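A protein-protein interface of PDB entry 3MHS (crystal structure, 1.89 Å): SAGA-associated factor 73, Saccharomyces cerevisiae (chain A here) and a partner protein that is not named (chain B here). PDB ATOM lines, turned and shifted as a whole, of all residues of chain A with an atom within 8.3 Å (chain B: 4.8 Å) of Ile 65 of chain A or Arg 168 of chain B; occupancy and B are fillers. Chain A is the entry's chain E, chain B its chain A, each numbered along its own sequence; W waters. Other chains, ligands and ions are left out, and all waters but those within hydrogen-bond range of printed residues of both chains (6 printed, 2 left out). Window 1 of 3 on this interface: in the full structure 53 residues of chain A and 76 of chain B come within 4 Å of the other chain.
The side-chain hydroxyl (OG) of Ser 172 of chain B is in hydrogen-bond range of the backbone carbonyl oxygen (O) of Arg 168 of chain B (2.7 Å).
Of the 21 printed residues of chain A, 9 touch a printed residue of chain B.
Printed residues of chain A that touch a printed residue of chain B: Gln 63, Leu 64, Ile 65, Pro 68, Ile 73, Pro 84, Leu 85, Ala 86 and Ala 89.
Of the 10 printed residues of chain B, 6 touch a printed residue of chain A.
Printed residues of chain B that touch a printed residue of chain A: Pro 164, Tyr 165, Ile 167, Arg 168, Met 171 and Ser 172.
Hydrophobic or aromatic side chains of chain B within 4 Å of the printed part of chain A: Pro 164, Tyr 165, Ile 167 and Met 171.
Among the printed residues, 14 pairs touch across the chains.
Ile 65 of chain A touches three residues of chain B.
Arg 168 of chain B touches two residues of chain A.
Printed residues of chain B within 4 Å of Pro 68 of chain A: Pro 164.
Of the printed residues of chain B, Pro 84 of chain A touches Met 171 (3.6 Å).
His 169 of chain B touches none of the printed residues of chain A.
The nearest residue of chain A that does not touch Arg 168 of chain B is Leu 64 of chain A (4.1 Å).
The backbone NH (N) of Ala 86 of chain A lies within hydrogen-bond range of the backbone carbonyl oxygen (O) of Met 171 of chain B, at 3.0 Å.
NH2 of Arg 168 of chain B lies within hydrogen-bond range of OE1 of Gln 63 of chain A (3.1 Å).
The backbone NH (N) of Ile 65 of chain A sits at hydrogen-bond distance from the side-chain hydroxyl (OH) of Tyr 165 of chain B (2.9 Å).
CE1 of Tyr 165 of chain B touches O of Gln 63 of chain A (3.5 Å).
Leu 64 of chain A touches Tyr 165 of chain B.
Ile 65 of chain A touches Pro 164 of chain B.
Ile 65 of chain A touches Arg 168 of chain B.
Pro 164 of chain B touches Pro 68 of chain A.
Ile 73 of chain A touches Ile 167 of chain B.
Met 171 of chain B touches Pro 84 of chain A.
Leu 85 of chain A touches Met 171 of chain B (CA to O, 3.6 Å).
Ser 172 of chain B touches Ala 86 of chain A (OG to CB, 3.5 Å).
Ala 89 of chain A touches Met 171 of chain B.
Water W3 lies within hydrogen-bond range of the side-chain hydroxyl (OH) of Tyr 165 of chain B (2.6 Å), the backbone carbonyl oxygen (O) of Ile 472 of chain B (2.7 Å) and the backbone carbonyl oxygen (O) of Ile 65 of chain A (2.9 Å).
Water W5 lies within hydrogen-bond range of OE1 of Gln 63 of chain A (2.6 Å), O of Tyr 165 of chain B (2.6 Å), NE of Arg 168 of chain B (2.9 Å) and N of His 169 of chain B (3.5 Å).
Water W4 bridges ND1 of His 169 of chain B (2.7 Å) and NE2 of Gln 63 of chain A (3.1 Å).
Water W1 lies within hydrogen-bond range of the backbone NH of Asp 67 of chain A (2.8 Å), the backbone carbonyl oxygen of Ile 472 of chain B (3.5 Å) and the side-chain sulfur of Met 49 of chain A (3.7 Å).
Water W6 bridges the side-chain hydroxyl of Thr 88 of chain A (2.9 Å) and the side-chain hydroxyl of Ser 172 of chain B (3.1 Å).
Water W2 lies within hydrogen-bond range of O of Gln 74 of chain A (2.9 Å) and SD of Met 171 of chain B (3.3 Å).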
ATOM      1  N   LEU A  44      -9.471  -3.298 -18.266  1.00  0.00           N
ATOM      2  CA  LEU A  44      -9.727  -2.965 -16.851  1.00  0.00           C
ATOM      3  C   LEU A  44      -8.474  -2.403 -16.168  1.00  0.00           C
ATOM      4  O   LEU A  44      -7.379  -2.954 -16.298  1.00  0.00           O
ATOM      5  CB  LEU A  44     -10.240  -4.220 -16.117  1.00  0.00           C
ATOM      6  CG  LEU A  44     -10.528  -4.122 -14.600  1.00  0.00           C
ATOM      7  CD1 LEU A  44     -11.805  -3.380 -14.385  1.00  0.00           C
ATOM      8  CD2 LEU A  44     -10.662  -5.557 -14.003  1.00  0.00           C
ATOM      9  N   TYR A  46      -6.831  -0.552 -12.506  1.00  0.00           N
ATOM     10  CA  TYR A  46      -6.964  -0.438 -11.035  1.00  0.00           C
ATOM     11  C   TYR A  46      -6.469   0.915 -10.593  1.00  0.00           C
ATOM     12  O   TYR A  46      -5.547   1.491 -11.185  1.00  0.00           O
ATOM     13  CB  TYR A  46      -6.174  -1.551 -10.343  1.00  0.00           C
ATOM     14  CG  TYR A  46      -6.589  -2.921 -10.801  1.00  0.00           C
ATOM     15  CD1 TYR A  46      -7.789  -3.500 -10.365  1.00  0.00           C
ATOM     16  CD2 TYR A  46      -5.823  -3.628 -11.727  1.00  0.00           C
ATOM     17  CE1 TYR A  46      -8.180  -4.749 -10.792  1.00  0.00           C
ATOM     18  CE2 TYR A  46      -6.236  -4.865 -12.203  1.00  0.00           C
ATOM     19  CZ  TYR A  46      -7.397  -5.432 -11.691  1.00  0.00           C
ATOM     20  OH  TYR A  46      -7.802  -6.640 -12.165  1.00  0.00           O
ATOM     21  N   HIS A  48      -4.918   1.605  -7.725  1.00  0.00           N
ATOM     22  CA  HIS A  48      -3.606   1.556  -7.078  1.00  0.00           C
ATOM     23  C   HIS A  48      -2.952   0.178  -7.194  1.00  0.00           C
ATOM     24  O   HIS A  48      -2.299  -0.293  -6.273  1.00  0.00           O
ATOM     25  CB  HIS A  48      -3.660   2.038  -5.613  1.00  0.00           C
ATOM     26  CG  HIS A  48      -4.807   1.476  -4.836  1.00  0.00           C
ATOM     27  ND1 HIS A  48      -6.035   2.107  -4.762  1.00  0.00           N
ATOM     28  CD2 HIS A  48      -4.920   0.338  -4.107  1.00  0.00           C
ATOM     29  CE1 HIS A  48      -6.856   1.373  -4.030  1.00  0.00           C
ATOM     30  NE2 HIS A  48      -6.202   0.299  -3.614  1.00  0.00           N
ATOM     31  N   MET A  49      -3.158  -0.456  -8.336  1.00  0.00           N
ATOM     32  CA  MET A  49      -2.333  -1.555  -8.756  1.00  0.00           C
ATOM     33  C   MET A  49      -1.881  -1.273 -10.172  1.00  0.00           C
ATOM     34  O   MET A  49      -2.592  -1.495 -11.172  1.00  0.00           O
ATOM     35  CB  MET A  49      -3.057  -2.898  -8.594  1.00  0.00           C
ATOM     36  CG  MET A  49      -3.486  -3.148  -7.154  1.00  0.00           C
ATOM     37  SD  MET A  49      -3.964  -4.860  -6.862  1.00  0.00           S
ATOM     38  CE  MET A  49      -5.408  -4.934  -7.873  1.00  0.00           C
ATOM     39  N   ALA A  62      -2.995 -13.922 -13.124  1.00  0.00           N
ATOM     40  CA  ALA A  62      -3.283 -13.704 -11.734  1.00  0.00           C
ATOM     41  C   ALA A  62      -4.727 -13.213 -11.576  1.00  0.00           C
ATOM     42  O   ALA A  62      -5.185 -12.318 -12.318  1.00  0.00           O
ATOM     43  CB  ALA A  62      -2.311 -12.683 -11.147  1.00  0.00           C
ATOM     44  N   GLN A  63      -5.445 -13.762 -10.591  1.00  0.00           N
ATOM     45  CA  GLN A  63      -6.743 -13.157 -10.193  1.00  0.00           C
ATOM     46  C   GLN A  63      -6.423 -11.916  -9.373  1.00  0.00           C
ATOM     47  O   GLN A  63      -5.502 -11.917  -8.554  1.00  0.00           O
ATOM     48  CB  GLN A  63      -7.608 -14.121  -9.367  1.00  0.00           C
ATOM     49  CG  GLN A  63      -8.130 -15.271 -10.157  1.00  0.00           C
ATOM     50  CD  GLN A  63      -9.265 -16.003  -9.471  1.00  0.00           C
ATOM     51  OE1 GLN A  63      -9.933 -15.449  -8.584  1.00  0.00           O
ATOM     52  NE2 GLN A  63      -9.460 -17.283  -9.845  1.00  0.00           N
ATOM     53  N   LEU A  64      -7.179 -10.841  -9.555  1.00  0.00           N
ATOM     54  CA  LEU A  64      -6.914  -9.641  -8.766  1.00  0.00           C
ATOM     55  C   LEU A  64      -8.202  -9.012  -8.306  1.00  0.00           C
ATOM     56  O   LEU A  64      -9.130  -8.848  -9.101  1.00  0.00           O
ATOM     57  CB  LEU A  64      -6.099  -8.654  -9.594  1.00  0.00           C
ATOM     58  CG  LEU A  64      -4.669  -9.050  -9.977  1.00  0.00           C
ATOM     59  CD1 LEU A  64      -4.137  -8.068 -11.060  1.00  0.00           C
ATOM     60  CD2 LEU A  64      -3.731  -9.006  -8.734  1.00  0.00           C
ATOM     61  N   ILE A  65      -8.289  -8.776  -7.003  1.00  0.00           N
ATOM     62  CA  ILE A  65      -9.371  -8.033  -6.407  1.00  0.00           C
ATOM     63  C   ILE A  65      -8.763  -6.813  -5.775  1.00  0.00           C
ATOM     64  O   ILE A  65      -7.945  -6.927  -4.891  1.00  0.00           O
ATOM     65  CB  ILE A  65     -10.126  -8.835  -5.330  1.00  0.00           C
ATOM     66  CG1 ILE A  65     -10.855 -10.044  -5.958  1.00  0.00           C
ATOM     67  CG2 ILE A  65     -11.222  -7.904  -4.648  1.00  0.00           C
ATOM     68  CD1 ILE A  65     -11.244 -11.148  -4.953  1.00  0.00           C
ATOM     69  N   GLU A  66      -9.118  -5.630  -6.254  1.00  0.00           N
ATOM     70  CA  GLU A  66      -8.620  -4.413  -5.624  1.00  0.00           C
ATOM     71  C   GLU A  66      -9.390  -4.159  -4.316  1.00  0.00           C
ATOM     72  O   GLU A  66     -10.658  -4.181  -4.296  1.00  0.00           O
ATOM     73  CB  GLU A  66      -8.749  -3.176  -6.537  1.00  0.00           C
ATOM     74  CG  GLU A  66      -8.100  -1.909  -5.914  1.00  0.00           C
ATOM     75  CD  GLU A  66      -7.617  -0.865  -6.940  1.00  0.00           C
ATOM     76  OE1 GLU A  66      -8.436  -0.477  -7.779  1.00  0.00           O
ATOM     77  OE2 GLU A  66      -6.423  -0.455  -6.924  1.00  0.00           O
ATOM     78  N   ASP A  67      -8.618  -3.897  -3.259  1.00  0.00           N
ATOM     79  CA  ASP A  67      -9.129  -3.573  -1.925  1.00  0.00           C
ATOM     80  C   ASP A  67     -10.224  -4.569  -1.508  1.00  0.00           C
ATOM     81  O   ASP A  67     -11.390  -4.185  -1.316  1.00  0.00           O
ATOM     82  CB  ASP A  67      -9.674  -2.144  -1.888  1.00  0.00           C
ATOM     83  CG  ASP A  67      -8.622  -1.072  -2.213  1.00  0.00           C
ATOM     84  OD1 ASP A  67      -7.397  -1.338  -2.080  1.00  0.00           O
ATOM     85  OD2 ASP A  67      -9.048   0.036  -2.646  1.00  0.00           O
ATOM     86  N   PRO A  68      -9.856  -5.867  -1.384  1.00  0.00           N
ATOM     87  CA  PRO A  68     -10.853  -6.912  -1.164  1.00  0.00           C
ATOM     88  C   PRO A  68     -11.637  -6.747   0.142  1.00  0.00           C
ATOM     89  O   PRO A  68     -12.773  -7.236   0.230  1.00  0.00           O
ATOM     90  CB  PRO A  68     -10.051  -8.212  -1.202  1.00  0.00           C
ATOM     91  CG  PRO A  68      -8.638  -7.784  -0.868  1.00  0.00           C
ATOM     92  CD  PRO A  68      -8.486  -6.390  -1.379  1.00  0.00           C
ATOM     93  N   LEU A  69     -11.070  -6.046   1.119  1.00  0.00           N
ATOM     94  CA  LEU A  69     -11.762  -5.794   2.390  1.00  0.00           C
ATOM     95  C   LEU A  69     -12.364  -4.381   2.491  1.00  0.00           C
ATOM     96  O   LEU A  69     -12.690  -3.948   3.589  1.00  0.00           O
ATOM     97  CB  LEU A  69     -10.848  -6.047   3.616  1.00  0.00           C
ATOM     98  CG  LEU A  69     -10.734  -7.497   4.101  1.00  0.00           C
ATOM     99  CD1 LEU A  69     -10.275  -8.415   2.977  1.00  0.00           C
ATOM    100  CD2 LEU A  69      -9.825  -7.627   5.326  1.00  0.00           C
ATOM    101  N   ASP A  70     -12.518  -3.695   1.362  1.00  0.00           N
ATOM    102  CA  ASP A  70     -13.097  -2.344   1.341  1.00  0.00           C
ATOM    103  C   ASP A  70     -14.497  -2.361   1.967  1.00  0.00           C
ATOM    104  O   ASP A  70     -14.821  -1.553   2.834  1.00  0.00           O
ATOM    105  CB  ASP A  70     -13.198  -1.855  -0.093  1.00  0.00           C
ATOM    106  CG  ASP A  70     -13.742  -0.443  -0.196  1.00  0.00           C
ATOM    107  OD1 ASP A  70     -13.113   0.447   0.400  1.00  0.00           O
ATOM    108  OD2 ASP A  70     -14.767  -0.237  -0.876  1.00  0.00           O
ATOM    109  N   ILE A  73     -18.605  -8.678   2.040  1.00  0.00           N
ATOM    110  CA  ILE A  73     -18.833  -9.549   0.887  1.00  0.00           C
ATOM    111  C   ILE A  73     -20.178  -9.218   0.252  1.00  0.00           C
ATOM    112  O   ILE A  73     -21.185  -9.095   0.969  1.00  0.00           O
ATOM    113  CB  ILE A  73     -18.826 -11.041   1.316  1.00  0.00           C
ATOM    114  CG1 ILE A  73     -17.539 -11.402   2.080  1.00  0.00           C
ATOM    115  CG2 ILE A  73     -19.029 -11.945   0.106  1.00  0.00           C
ATOM    116  CD1 ILE A  73     -16.211 -11.362   1.242  1.00  0.00           C
ATOM    117  N   GLN A  74     -20.175  -9.006  -1.064  1.00  0.00           N
ATOM    118  CA  GLN A  74     -21.367  -8.619  -1.834  1.00  0.00           C
ATOM    119  C   GLN A  74     -22.030  -9.854  -2.405  1.00  0.00           C
ATOM    120  O   GLN A  74     -21.442 -10.594  -3.199  1.00  0.00           O
ATOM    121  CB  GLN A  74     -21.020  -7.672  -2.972  1.00  0.00           C
ATOM    122  CG  GLN A  74     -20.324  -6.408  -2.495  1.00  0.00           C
ATOM    123  CD  GLN A  74     -21.242  -5.536  -1.690  1.00  0.00           C
ATOM    124  OE1 GLN A  74     -22.217  -5.024  -2.231  1.00  0.00           O
ATOM    125  NE2 GLN A  74     -20.938  -5.342  -0.387  1.00  0.00           N
ATOM    126  N   PRO A  84     -25.635 -18.687  -1.158  1.00  0.00           N
ATOM    127  CA  PRO A  84     -25.093 -17.344  -1.319  1.00  0.00           C
ATOM    128  C   PRO A  84     -24.512 -17.163  -2.713  1.00  0.00           C
ATOM    129  O   PRO A  84     -23.602 -17.921  -3.105  1.00  0.00           O
ATOM    130  CB  PRO A  84     -24.002 -17.258  -0.237  1.00  0.00           C
ATOM    131  CG  PRO A  84     -23.630 -18.613   0.078  1.00  0.00           C
ATOM    132  CD  PRO A  84     -24.744 -19.557  -0.387  1.00  0.00           C
ATOM    133  N   LEU A  85     -24.990 -16.163  -3.447  1.00  0.00           N
ATOM    134  CA  LEU A  85     -24.623 -15.960  -4.861  1.00  0.00           C
ATOM    135  C   LEU A  85     -23.939 -14.633  -5.062  1.00  0.00           C
ATOM    136  O   LEU A  85     -24.453 -13.596  -4.624  1.00  0.00           O
ATOM    137  CB  LEU A  85     -25.885 -15.971  -5.718  1.00  0.00           C
ATOM    138  CG  LEU A  85     -26.715 -17.241  -5.681  1.00  0.00           C
ATOM    139  CD1 LEU A  85     -28.153 -16.994  -6.208  1.00  0.00           C
ATOM    140  CD2 LEU A  85     -26.028 -18.349  -6.447  1.00  0.00           C
ATOM    141  N   ALA A  86     -22.789 -14.641  -5.741  1.00  0.00           N
ATOM    142  CA  ALA A  86     -22.171 -13.388  -6.179  1.00  0.00           C
ATOM    143  C   ALA A  86     -23.177 -12.710  -7.090  1.00  0.00           C
ATOM    144  O   ALA A  86     -23.912 -13.381  -7.827  1.00  0.00           O
ATOM    145  CB  ALA A  86     -20.879 -13.658  -6.958  1.00  0.00           C
ATOM    146  N   LEU A  87     -23.152 -11.384  -7.112  1.00  0.00           N
ATOM    147  CA  LEU A  87     -24.113 -10.644  -7.911  1.00  0.00           C
ATOM    148  C   LEU A  87     -24.014 -11.032  -9.403  1.00  0.00           C
ATOM    149  O   LEU A  87     -25.026 -11.081 -10.093  1.00  0.00           O
ATOM    150  CB  LEU A  87     -23.896  -9.138  -7.704  1.00  0.00           C
ATOM    151  CG  LEU A  87     -24.589  -8.511  -6.474  1.00  0.00           C
ATOM    152  CD1 LEU A  87     -26.017  -8.080  -6.811  1.00  0.00           C
ATOM    153  CD2 LEU A  87     -24.616  -9.437  -5.289  1.00  0.00           C
ATOM    154  N   THR A  88     -22.813 -11.346  -9.885  1.00  0.00           N
ATOM    155  CA  THR A  88     -22.633 -11.738 -11.280  1.00  0.00           C
ATOM    156  C   THR A  88     -23.098 -13.162 -11.568  1.00  0.00           C
ATOM    157  O   THR A  88     -23.197 -13.550 -12.726  1.00  0.00           O
ATOM    158  CB  THR A  88     -21.192 -11.508 -11.754  1.00  0.00           C
ATOM    159  OG1 THR A  88     -20.260 -12.119 -10.852  1.00  0.00           O
ATOM    160  CG2 THR A  88     -20.882  -9.994 -11.831  1.00  0.00           C
ATOM    161  N   ALA A  89     -23.466 -13.920 -10.537  1.00  0.00           N
ATOM    162  CA  ALA A  89     -23.932 -15.295 -10.716  1.00  0.00           C
ATOM    163  C   ALA A  89     -25.441 -15.488 -10.563  1.00  0.00           C
ATOM    164  O   ALA A  89     -25.934 -16.585 -10.756  1.00  0.00           O
ATOM    165  CB  ALA A  89     -23.212 -16.230  -9.747  1.00  0.00           C
ATOM    166  N   PRO B 164     -10.864 -13.654   0.475  1.00  0.00           N
ATOM    167  CA  PRO B 164     -11.754 -12.994  -0.508  1.00  0.00           C
ATOM    168  C   PRO B 164     -11.724 -13.648  -1.899  1.00  0.00           C
ATOM    169  O   PRO B 164     -12.735 -13.580  -2.629  1.00  0.00           O
ATOM    170  CB  PRO B 164     -11.170 -11.585  -0.640  1.00  0.00           C
ATOM    171  CG  PRO B 164      -9.825 -11.635  -0.041  1.00  0.00           C
ATOM    172  CD  PRO B 164      -9.805 -12.758   0.961  1.00  0.00           C
ATOM    173  N   TYR B 165     -10.601 -14.263  -2.271  1.00  0.00           N
ATOM    174  CA  TYR B 165     -10.513 -14.904  -3.582  1.00  0.00           C
ATOM    175  C   TYR B 165     -11.312 -16.207  -3.594  1.00  0.00           C
ATOM    176  O   TYR B 165     -12.021 -16.483  -4.572  1.00  0.00           O
ATOM    177  CB  TYR B 165      -9.063 -15.135  -4.064  1.00  0.00           C
ATOM    178  CG  TYR B 165      -8.322 -13.864  -4.371  1.00  0.00           C
ATOM    179  CD1 TYR B 165      -8.342 -13.331  -5.641  1.00  0.00           C
ATOM    180  CD2 TYR B 165      -7.670 -13.153  -3.373  1.00  0.00           C
ATOM    181  CE1 TYR B 165      -7.723 -12.130  -5.913  1.00  0.00           C
ATOM    182  CE2 TYR B 165      -7.014 -11.943  -3.652  1.00  0.00           C
ATOM    183  CZ  TYR B 165      -7.069 -11.437  -4.925  1.00  0.00           C
ATOM    184  OH  TYR B 165      -6.461 -10.249  -5.266  1.00  0.00           O
ATOM    185  N   PHE B 166     -11.195 -17.002  -2.514  1.00  0.00           N
ATOM    186  CA  PHE B 166     -11.937 -18.222  -2.408  1.00  0.00           C
ATOM    187  C   PHE B 166     -13.424 -17.979  -2.253  1.00  0.00           C
ATOM    188  O   PHE B 166     -14.220 -18.660  -2.860  1.00  0.00           O
ATOM    189  CB  PHE B 166     -11.479 -19.142  -1.261  1.00  0.00           C
ATOM    190  CG  PHE B 166     -12.151 -20.472  -1.317  1.00  0.00           C
ATOM    191  CD1 PHE B 166     -11.829 -21.374  -2.311  1.00  0.00           C
ATOM    192  CD2 PHE B 166     -13.212 -20.759  -0.460  1.00  0.00           C
ATOM    193  CE1 PHE B 166     -12.560 -22.579  -2.470  1.00  0.00           C
ATOM    194  CE2 PHE B 166     -13.879 -21.964  -0.557  1.00  0.00           C
ATOM    195  CZ  PHE B 166     -13.573 -22.863  -1.557  1.00  0.00           C
ATOM    196  N   ILE B 167     -13.759 -17.020  -1.388  1.00  0.00           N
ATOM    197  CA  ILE B 167     -15.124 -16.509  -1.218  1.00  0.00           C
ATOM    198  C   ILE B 167     -15.795 -16.245  -2.575  1.00  0.00           C
ATOM    199  O   ILE B 167     -16.859 -16.809  -2.896  1.00  0.00           O
ATOM    200  CB  ILE B 167     -15.111 -15.220  -0.299  1.00  0.00           C
ATOM    201  CG1 ILE B 167     -15.030 -15.694   1.161  1.00  0.00           C
ATOM    202  CG2 ILE B 167     -16.323 -14.330  -0.573  1.00  0.00           C
ATOM    203  CD1 ILE B 167     -14.792 -14.594   2.264  1.00  0.00           C
ATOM    204  N   ARG B 168     -15.151 -15.422  -3.382  1.00  0.00           N
ATOM    205  CA  ARG B 168     -15.674 -14.982  -4.693  1.00  0.00           C
ATOM    206  C   ARG B 168     -15.824 -16.186  -5.662  1.00  0.00           C
ATOM    207  O   ARG B 168     -16.862 -16.342  -6.316  1.00  0.00           O
ATOM    208  CB  ARG B 168     -14.776 -13.909  -5.298  1.00  0.00           C
ATOM    209  CG  ARG B 168     -15.163 -13.525  -6.719  1.00  0.00           C
ATOM    210  CD  ARG B 168     -14.361 -12.412  -7.288  1.00  0.00           C
ATOM    211  NE  ARG B 168     -13.026 -12.843  -7.726  1.00  0.00           N
ATOM    212  CZ  ARG B 168     -12.255 -12.130  -8.526  1.00  0.00           C
ATOM    213  NH1 ARG B 168     -12.649 -10.937  -8.934  1.00  0.00           N
ATOM    214  NH2 ARG B 168     -11.089 -12.603  -8.935  1.00  0.00           N
ATOM    215  N   HIS B 169     -14.820 -17.071  -5.677  1.00  0.00           N
ATOM    216  CA  HIS B 169     -14.857 -18.326  -6.438  1.00  0.00           C
ATOM    217  C   HIS B 169     -16.046 -19.183  -6.097  1.00  0.00           C
ATOM    218  O   HIS B 169     -16.791 -19.613  -6.983  1.00  0.00           O
ATOM    219  CB  HIS B 169     -13.549 -19.105  -6.186  1.00  0.00           C
ATOM    220  CG  HIS B 169     -13.477 -20.430  -6.860  1.00  0.00           C
ATOM    221  ND1 HIS B 169     -13.289 -20.562  -8.219  1.00  0.00           N
ATOM    222  CD2 HIS B 169     -13.553 -21.689  -6.365  1.00  0.00           C
ATOM    223  CE1 HIS B 169     -13.243 -21.848  -8.533  1.00  0.00           C
ATOM    224  NE2 HIS B 169     -13.395 -22.551  -7.425  1.00  0.00           N
ATOM    225  N   SER B 170     -16.252 -19.431  -4.810  1.00  0.00           N
ATOM    226  CA  SER B 170     -17.307 -20.314  -4.369  1.00  0.00           C
ATOM    227  C   SER B 170     -18.692 -19.714  -4.650  1.00  0.00           C
ATOM    228  O   SER B 170     -19.554 -20.381  -5.185  1.00  0.00           O
ATOM    229  CB  SER B 170     -17.150 -20.637  -2.902  1.00  0.00           C
ATOM    230  OG  SER B 170     -18.156 -21.544  -2.502  1.00  0.00           O
ATOM    231  N   MET B 171     -18.864 -18.438  -4.336  1.00  0.00           N
ATOM    232  CA  MET B 171     -20.151 -17.768  -4.542  1.00  0.00           C
ATOM    233  C   MET B 171     -20.464 -17.497  -6.018  1.00  0.00           C
ATOM    234  O   MET B 171     -21.626 -17.324  -6.379  1.00  0.00           O
ATOM    235  CB  MET B 171     -20.198 -16.477  -3.739  1.00  0.00           C
ATOM    236  CG  MET B 171     -20.365 -16.730  -2.264  1.00  0.00           C
ATOM    237  SD  MET B 171     -20.923 -15.226  -1.437  1.00  0.00           S
ATOM    238  CE  MET B 171     -20.640 -15.667   0.294  1.00  0.00           C
ATOM    239  N   SER B 172     -19.441 -17.471  -6.864  1.00  0.00           N
ATOM    240  CA  SER B 172     -19.668 -17.314  -8.293  1.00  0.00           C
ATOM    241  C   SER B 172     -20.045 -18.647  -8.971  1.00  0.00           C
ATOM    242  O   SER B 172     -20.176 -18.703 -10.194  1.00  0.00           O
ATOM    243  CB  SER B 172     -18.459 -16.668  -8.978  1.00  0.00           C
ATOM    244  OG  SER B 172     -18.170 -15.386  -8.432  1.00  0.00           O
ATOM    245  N   ILE B 472      -2.856  -9.110  -1.723  1.00  0.00           N
ATOM    246  CA  ILE B 472      -2.258  -7.950  -2.386  1.00  0.00           C
ATOM    247  C   ILE B 472      -3.186  -6.748  -2.230  1.00  0.00           C
ATOM    248  O   ILE B 472      -4.422  -6.866  -2.389  1.00  0.00           O
ATOM    249  CB  ILE B 472      -1.856  -8.247  -3.867  1.00  0.00           C
ATOM    250  CG1 ILE B 472      -0.992  -7.114  -4.464  1.00  0.00           C
ATOM    251  CG2 ILE B 472      -3.122  -8.566  -4.776  1.00  0.00           C
ATOM    252  CD1 ILE B 472       0.383  -6.861  -3.715  1.00  0.00           C
HETATM  253  O   HOH W   1      -5.927  -4.066  -3.810  1.00  0.00           O
HETATM  254  O   HOH W   2     -19.547 -12.841  -3.301  1.00  0.00           O
HETATM  255  O   HOH W   3      -6.241  -8.649  -3.254  1.00  0.00           O
HETATM  256  O   HOH W   4     -12.219 -18.655  -9.813  1.00  0.00           O
HETATM  257  O   HOH W   5     -12.032 -15.495  -7.023  1.00  0.00           O
HETATM  258  O   HOH W   6     -17.910 -12.355  -9.130  1.00  0.00           O
